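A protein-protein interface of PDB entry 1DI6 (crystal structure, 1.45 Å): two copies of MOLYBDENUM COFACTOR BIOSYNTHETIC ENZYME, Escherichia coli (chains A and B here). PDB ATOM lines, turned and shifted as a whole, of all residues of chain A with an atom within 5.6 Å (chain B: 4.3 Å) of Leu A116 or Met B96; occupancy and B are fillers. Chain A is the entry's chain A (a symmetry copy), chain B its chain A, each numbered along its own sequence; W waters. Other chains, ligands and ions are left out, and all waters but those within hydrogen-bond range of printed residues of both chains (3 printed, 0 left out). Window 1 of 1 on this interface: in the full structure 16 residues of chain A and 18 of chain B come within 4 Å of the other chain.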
ATOM      1  N   THR A  76     -24.565 -18.865  11.607  1.00  0.00           N
ATOM      2  CA  THR A  76     -25.831 -19.265  10.970  1.00  0.00           C
ATOM      3  C   THR A  76     -25.770 -19.383   9.470  1.00  0.00           C
ATOM      4  O   THR A  76     -26.831 -19.562   8.856  1.00  0.00           O
ATOM      5  CB  THR A  76     -26.976 -18.290  11.310  1.00  0.00           C
ATOM      6  OG1 THR A  76     -26.701 -17.021  10.712  1.00  0.00           O
ATOM      7  CG2 THR A  76     -27.201 -18.177  12.806  1.00  0.00           C
ATOM      8  N   GLY A  77     -24.625 -19.295   8.802  1.00  0.00           N
ATOM      9  CA  GLY A  77     -24.567 -19.413   7.346  1.00  0.00           C
ATOM     10  C   GLY A  77     -24.536 -20.842   6.803  1.00  0.00           C
ATOM     11  O   GLY A  77     -24.705 -21.807   7.536  1.00  0.00           O
ATOM     12  N   PRO A  78     -24.139 -20.979   5.535  1.00  0.00           N
ATOM     13  CA  PRO A  78     -24.147 -22.232   4.806  1.00  0.00           C
ATOM     14  C   PRO A  78     -22.887 -23.076   4.978  1.00  0.00           C
ATOM     15  O   PRO A  78     -22.913 -24.266   4.696  1.00  0.00           O
ATOM     16  CB  PRO A  78     -24.202 -21.809   3.304  1.00  0.00           C
ATOM     17  CG  PRO A  78     -23.504 -20.479   3.328  1.00  0.00           C
ATOM     18  CD  PRO A  78     -23.884 -19.827   4.657  1.00  0.00           C
ATOM     19  N   PRO A 112     -29.076  -9.002  -0.430  1.00  0.00           N
ATOM     20  CA  PRO A 112     -29.733 -10.177  -0.958  1.00  0.00           C
ATOM     21  C   PRO A 112     -29.207 -11.480  -0.382  1.00  0.00           C
ATOM     22  O   PRO A 112     -29.913 -12.498  -0.374  1.00  0.00           O
ATOM     23  CB  PRO A 112     -29.576 -10.116  -2.498  1.00  0.00           C
ATOM     24  CG  PRO A 112     -28.490  -9.082  -2.683  1.00  0.00           C
ATOM     25  CD  PRO A 112     -28.409  -8.194  -1.469  1.00  0.00           C
ATOM     26  N   THR A 113     -27.980 -11.485   0.123  1.00  0.00           N
ATOM     27  CA  THR A 113     -27.330 -12.640   0.696  1.00  0.00           C
ATOM     28  C   THR A 113     -27.860 -13.074   2.046  1.00  0.00           C
ATOM     29  O   THR A 113     -27.490 -14.128   2.584  1.00  0.00           O
ATOM     30  CB  THR A 113     -25.799 -12.494   0.731  1.00  0.00           C
ATOM     31  OG1 THR A 113     -25.511 -11.188   1.292  1.00  0.00           O
ATOM     32  CG2 THR A 113     -25.219 -12.549  -0.682  1.00  0.00           C
ATOM     33  N   ALA A 114     -28.832 -12.314   2.593  1.00  0.00           N
ATOM     34  CA  ALA A 114     -29.553 -12.747   3.796  1.00  0.00           C
ATOM     35  C   ALA A 114     -30.218 -14.085   3.641  1.00  0.00           C
ATOM     36  O   ALA A 114     -30.354 -14.745   4.694  1.00  0.00           O
ATOM     37  CB  ALA A 114     -30.670 -11.696   4.041  1.00  0.00           C
ATOM     38  N   ILE A 115     -30.533 -14.475   2.415  1.00  0.00           N
ATOM     39  CA  ILE A 115     -31.153 -15.791   2.268  1.00  0.00           C
ATOM     40  C   ILE A 115     -30.196 -16.948   2.517  1.00  0.00           C
ATOM     41  O   ILE A 115     -30.645 -18.089   2.562  1.00  0.00           O
ATOM     42  CB  ILE A 115     -31.864 -15.942   0.932  1.00  0.00           C
ATOM     43  CG1 ILE A 115     -30.845 -15.859  -0.197  1.00  0.00           C
ATOM     44  CG2 ILE A 115     -32.963 -14.897   0.778  1.00  0.00           C
ATOM     45  CD1 ILE A 115     -31.466 -16.423  -1.477  1.00  0.00           C
ATOM     46  N   LEU A 116     -28.897 -16.677   2.673  1.00  0.00           N
ATOM     47  CA  LEU A 116     -27.957 -17.755   2.983  1.00  0.00           C
ATOM     48  C   LEU A 116     -27.965 -18.109   4.452  1.00  0.00           C
ATOM     49  O   LEU A 116     -27.259 -19.019   4.932  1.00  0.00           O
ATOM     50  CB  LEU A 116     -26.566 -17.375   2.476  1.00  0.00           C
ATOM     51  CG  LEU A 116     -26.376 -17.062   1.008  1.00  0.00           C
ATOM     52  CD1 LEU A 116     -24.893 -16.783   0.679  1.00  0.00           C
ATOM     53  CD2 LEU A 116     -26.877 -18.172   0.084  1.00  0.00           C
ATOM     54  N   SER A 117     -28.630 -17.302   5.319  1.00  0.00           N
ATOM     55  CA  SER A 117     -28.716 -17.631   6.747  1.00  0.00           C
ATOM     56  C   SER A 117     -29.728 -18.710   7.025  1.00  0.00           C
ATOM     57  O   SER A 117     -30.820 -18.823   6.436  1.00  0.00           O
ATOM     58  CB  SER A 117     -29.069 -16.440   7.657  1.00  0.00           C
ATOM     59  OG  SER A 117     -29.217 -16.847   9.033  1.00  0.00           O
ATOM     60  N   ARG A 118     -29.422 -19.606   7.957  1.00  0.00           N
ATOM     61  CA  ARG A 118     -30.254 -20.719   8.361  1.00  0.00           C
ATOM     62  C   ARG A 118     -30.848 -20.516   9.776  1.00  0.00           C
ATOM     63  O   ARG A 118     -31.359 -21.426  10.400  1.00  0.00           O
ATOM     64  CB  ARG A 118     -29.461 -22.041   8.337  1.00  0.00           C
ATOM     65  CG  ARG A 118     -28.931 -22.426   6.977  1.00  0.00           C
ATOM     66  CD  ARG A 118     -28.077 -23.690   6.893  1.00  0.00           C
ATOM     67  NE  ARG A 118     -28.697 -24.877   7.413  1.00  0.00           N
ATOM     68  CZ  ARG A 118     -28.538 -25.514   8.567  1.00  0.00           C
ATOM     69  NH1 ARG A 118     -27.663 -25.063   9.448  1.00  0.00           N
ATOM     70  NH2 ARG A 118     -29.196 -26.619   8.885  1.00  0.00           N
ATOM     71  N   ARG B  94     -27.891 -30.925   4.480  1.00  0.00           N
ATOM     72  CA  ARG B  94     -28.440 -29.778   5.206  1.00  0.00           C
ATOM     73  C   ARG B  94     -29.390 -28.979   4.323  1.00  0.00           C
ATOM     74  O   ARG B  94     -29.154 -28.857   3.126  1.00  0.00           O
ATOM     75  CB  ARG B  94     -27.215 -28.955   5.637  1.00  0.00           C
ATOM     76  CG  ARG B  94     -27.246 -27.458   5.544  1.00  0.00           C
ATOM     77  CD  ARG B  94     -25.956 -26.776   5.936  1.00  0.00           C
ATOM     78  NE  ARG B  94     -25.481 -27.049   7.276  1.00  0.00           N
ATOM     79  CZ  ARG B  94     -24.695 -26.195   7.950  1.00  0.00           C
ATOM     80  NH1 ARG B  94     -24.346 -25.028   7.399  1.00  0.00           N
ATOM     81  NH2 ARG B  94     -24.311 -26.543   9.177  1.00  0.00           N
ATOM     82  N   GLU B  95     -30.428 -28.391   4.894  1.00  0.00           N
ATOM     83  CA  GLU B  95     -31.357 -27.549   4.168  1.00  0.00           C
ATOM     84  C   GLU B  95     -30.964 -26.067   4.283  1.00  0.00           C
ATOM     85  O   GLU B  95     -30.436 -25.608   5.297  1.00  0.00           O
ATOM     86  CB  GLU B  95     -32.789 -27.732   4.698  1.00  0.00           C
ATOM     87  CG  GLU B  95     -33.137 -29.204   4.885  1.00  0.00           C
ATOM     88  CD  GLU B  95     -34.459 -29.496   5.549  1.00  0.00           C
ATOM     89  OE1 GLU B  95     -35.378 -28.658   5.494  1.00  0.00           O
ATOM     90  OE2 GLU B  95     -34.591 -30.599   6.125  1.00  0.00           O
ATOM     91  N   MET B  96     -31.270 -25.296   3.279  1.00  0.00           N
ATOM     92  CA  MET B  96     -31.058 -23.834   3.224  1.00  0.00           C
ATOM     93  C   MET B  96     -32.459 -23.225   3.095  1.00  0.00           C
ATOM     94  O   MET B  96     -32.926 -23.027   1.971  1.00  0.00           O
ATOM     95  CB  MET B  96     -30.226 -23.469   1.962  1.00  0.00           C
ATOM     96  CG  MET B  96     -28.789 -23.995   2.051  1.00  0.00           C
ATOM     97  SD  MET B  96     -27.824 -23.173   3.311  1.00  0.00           S
ATOM     98  CE  MET B  96     -27.795 -21.508   2.653  1.00  0.00           C
ATOM     99  N   PRO B  97     -33.157 -22.983   4.200  1.00  0.00           N
ATOM    100  CA  PRO B  97     -34.566 -22.579   4.136  1.00  0.00           C
ATOM    101  C   PRO B  97     -34.848 -21.304   3.367  1.00  0.00           C
ATOM    102  O   PRO B  97     -35.909 -21.169   2.717  1.00  0.00           O
ATOM    103  CB  PRO B  97     -34.992 -22.451   5.624  1.00  0.00           C
ATOM    104  CG  PRO B  97     -33.674 -22.114   6.285  1.00  0.00           C
ATOM    105  CD  PRO B  97     -32.688 -23.073   5.575  1.00  0.00           C
ATOM    106  N   GLY B  98     -33.878 -20.375   3.352  1.00  0.00           N
ATOM    107  CA  GLY B  98     -34.011 -19.100   2.658  1.00  0.00           C
ATOM    108  C   GLY B  98     -34.192 -19.210   1.167  1.00  0.00           C
ATOM    109  O   GLY B  98     -34.812 -18.416   0.485  1.00  0.00           O
ATOM    110  N   PHE B  99     -33.557 -20.285   0.577  1.00  0.00           N
ATOM    111  CA  PHE B  99     -33.725 -20.451  -0.865  1.00  0.00           C
ATOM    112  C   PHE B  99     -35.141 -20.825  -1.273  1.00  0.00           C
ATOM    113  O   PHE B  99     -35.661 -20.158  -2.180  1.00  0.00           O
ATOM    114  CB  PHE B  99     -32.706 -21.502  -1.410  1.00  0.00           C
ATOM    115  CG  PHE B  99     -31.345 -20.950  -1.726  1.00  0.00           C
ATOM    116  CD1 PHE B  99     -30.236 -21.369  -1.017  1.00  0.00           C
ATOM    117  CD2 PHE B  99     -31.157 -20.088  -2.778  1.00  0.00           C
ATOM    118  CE1 PHE B  99     -28.967 -20.911  -1.344  1.00  0.00           C
ATOM    119  CE2 PHE B  99     -29.887 -19.583  -3.127  1.00  0.00           C
ATOM    120  CZ  PHE B  99     -28.814 -19.994  -2.370  1.00  0.00           C
ATOM    121  N   GLY B 100     -35.784 -21.784  -0.620  1.00  0.00           N
ATOM    122  CA  GLY B 100     -37.176 -22.090  -0.933  1.00  0.00           C
ATOM    123  C   GLY B 100     -38.081 -20.855  -0.720  1.00  0.00           C
ATOM    124  O   GLY B 100     -38.990 -20.516  -1.505  1.00  0.00           O
ATOM    125  N   GLY B 121     -33.825 -25.503  -1.552  1.00  0.00           N
ATOM    126  CA  GLY B 121     -32.378 -25.380  -1.804  1.00  0.00           C
ATOM    127  C   GLY B 121     -31.730 -26.179  -0.671  1.00  0.00           C
ATOM    128  O   GLY B 121     -32.125 -26.128   0.508  1.00  0.00           O
ATOM    129  N   ILE B 123     -27.790 -28.446   0.629  1.00  0.00           N
ATOM    130  CA  ILE B 123     -26.370 -28.754   0.393  1.00  0.00           C
ATOM    131  C   ILE B 123     -26.172 -30.266   0.600  1.00  0.00           C
ATOM    132  O   ILE B 123     -26.717 -30.901   1.489  1.00  0.00           O
ATOM    133  CB  ILE B 123     -25.486 -27.975   1.361  1.00  0.00           C
ATOM    134  CG1 ILE B 123     -25.570 -26.454   1.096  1.00  0.00           C
ATOM    135  CG2 ILE B 123     -24.000 -28.394   1.291  1.00  0.00           C
ATOM    136  CD1 ILE B 123     -25.161 -25.642   2.300  1.00  0.00           C
ATOM    137  N   SER B 161     -27.044 -14.422  -4.949  1.00  0.00           N
ATOM    138  CA  SER B 161     -26.355 -14.936  -3.770  1.00  0.00           C
ATOM    139  C   SER B 161     -25.601 -16.229  -4.058  1.00  0.00           C
ATOM    140  O   SER B 161     -24.890 -16.690  -3.151  1.00  0.00           O
ATOM    141  CB  SER B 161     -27.390 -15.218  -2.656  1.00  0.00           C
ATOM    142  OG  SER B 161     -28.030 -13.968  -2.334  1.00  0.00           O
ATOM    143  N   TYR B 164     -21.399 -16.063  -4.001  1.00  0.00           N
ATOM    144  CA  TYR B 164     -20.875 -16.071  -2.636  1.00  0.00           C
ATOM    145  C   TYR B 164     -21.150 -17.380  -1.895  1.00  0.00           C
ATOM    146  O   TYR B 164     -20.285 -17.851  -1.147  1.00  0.00           O
ATOM    147  CB  TYR B 164     -21.462 -14.881  -1.847  1.00  0.00           C
ATOM    148  CG  TYR B 164     -20.928 -14.651  -0.459  1.00  0.00           C
ATOM    149  CD1 TYR B 164     -19.558 -14.685  -0.165  1.00  0.00           C
ATOM    150  CD2 TYR B 164     -21.834 -14.365   0.561  1.00  0.00           C
ATOM    151  CE1 TYR B 164     -19.149 -14.450   1.157  1.00  0.00           C
ATOM    152  CE2 TYR B 164     -21.413 -14.142   1.859  1.00  0.00           C
ATOM    153  CZ  TYR B 164     -20.059 -14.172   2.128  1.00  0.00           C
ATOM    154  OH  TYR B 164     -19.640 -13.941   3.431  1.00  0.00           O
ATOM    155  N   CYS B 165     -22.317 -18.013  -2.097  1.00  0.00           N
ATOM    156  CA  CYS B 165     -22.575 -19.288  -1.418  1.00  0.00           C
ATOM    157  C   CYS B 165     -21.549 -20.358  -1.837  1.00  0.00           C
ATOM    158  O   CYS B 165     -21.024 -21.080  -0.990  1.00  0.00           O
ATOM    159  CB  CYS B 165     -24.016 -19.754  -1.728  1.00  0.00           C
ATOM    160  SG  CYS B 165     -24.548 -21.131  -0.670  1.00  0.00           S
HETATM  161  O   HOH W   1     -27.155 -28.685   8.868  1.00  0.00           O
HETATM  162  O   HOH W   2     -30.951 -28.791   7.774  1.00  0.00           O
HETATM  163  O   HOH W   3     -31.124 -20.327   4.132  1.00  0.00           O
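N of Arg A118 is in hydrogen-bond range of O of Thr A76 (2.7 Å).
The backbone NH of Ile B123 lies within hydrogen-bond range of the backbone carbonyl oxygen of Arg B94, at 2.9 Å.
O of Gly B121 sits at hydrogen-bond distance from N of Met B96, at 3.0 Å.
Water W3 lies within hydrogen-bond range of the backbone carbonyl oxygen (O) of Ser A117 (2.8 Å), the backbone carbonyl oxygen (O) of Ile A115 (2.8 Å) and the backbone NH (N) of Gly B98 (2.9 Å).
Water W1 lies within hydrogen-bond range of the guanidinium group (NE) of Arg B94 and the guanidinium group (NH2) of Arg A118.
Water W2 bridges N of Glu B95 and NH2 of Arg A118.
Of chain B, only Met B96, Phe B99, Ser B161, Tyr B164 and Cys B165 come within 4 Å of Leu A116.
Met B96 touches three residues of chain A.
Of the printed residues of chain B, Pro A78 touches Arg B94, Met B96 and Ile B123.
Printed residues of chain A within 4 Å of Ser B161: Pro A112, Thr A113 and Leu A116.
Printed residues of chain A within 4 Å of Arg B94: Gly A77 (3.2 Å), Pro A78 (3.2 Å) and Arg A118 (3.5 Å).
Of the printed residues of chain B, Ile A115 touches Gly B98 and Phe B99.
No position is printed for both chains.
Of the 16 pairs that touch across the chains among the printed residues, none has its exchanged pair printed and touching as well.
O of Pro A78 touches CD1 of Ile B123 (3.6 Å).
CA of Gly B98 touches O of Ile A115, at 3.5 Å.
CE2 of Phe B99 touches CD1 of Ile A115, 3.9 Å away.
O of Leu A116 touches CE of Met B96 (3.4 Å).
Phe B99 touches Leu A116 (CZ to CD2, 3.6 Å).
O of Ser B161 touches CD1 of Leu A116, 3.8 Å away.
Tyr B164 touches Leu A116.
CB of Cys B165 touches CD2 of Leu A116, 3.7 Å away.
NE of Arg A118 touches CG of Arg B94, 3.5 Å away.
Met B96 touches Arg A118 (SD to CD, 3.6 Å).
Of the 12 printed residues of chain B, 9 touch a printed residue of chain A.
Hydrophobic or aromatic side chains of chain B within 4 Å of the printed part of chain A: Met B96, Phe B99, Ile B123 and Tyr B164.
Along chain B the printed residues that touch a printed residue of chain A span positions 94 to 165.
Of the 10 printed residues of chain A, 7 touch a printed residue of chain B.
Hydrophobic or aromatic side chains of chain A that line the printed part of chain B: Pro A78, Ile A115 and Leu A116.
The backbone carbonyl oxygen of Glu B95 lies within hydrogen-bond range of the guanidinium group of Arg A118 (2.8 Å).
The guanidinium group (NH1) of Arg B94 lies within hydrogen-bond range of the backbone carbonyl oxygen (O) of Pro A78.
The side-chain hydroxyl (OG) of Ser B161 sits at hydrogen-bond distance from the backbone carbonyl oxygen (O) of Pro A112 (3.1 Å).
The guanidinium group (NH1) of Arg B94 sits at hydrogen-bond distance from the backbone carbonyl oxygen (O) of Gly A77 (3.2 Å).
The side-chain hydroxyl of Ser B161 sits close to the backbone NH of Thr A113, 3.5 Å away.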
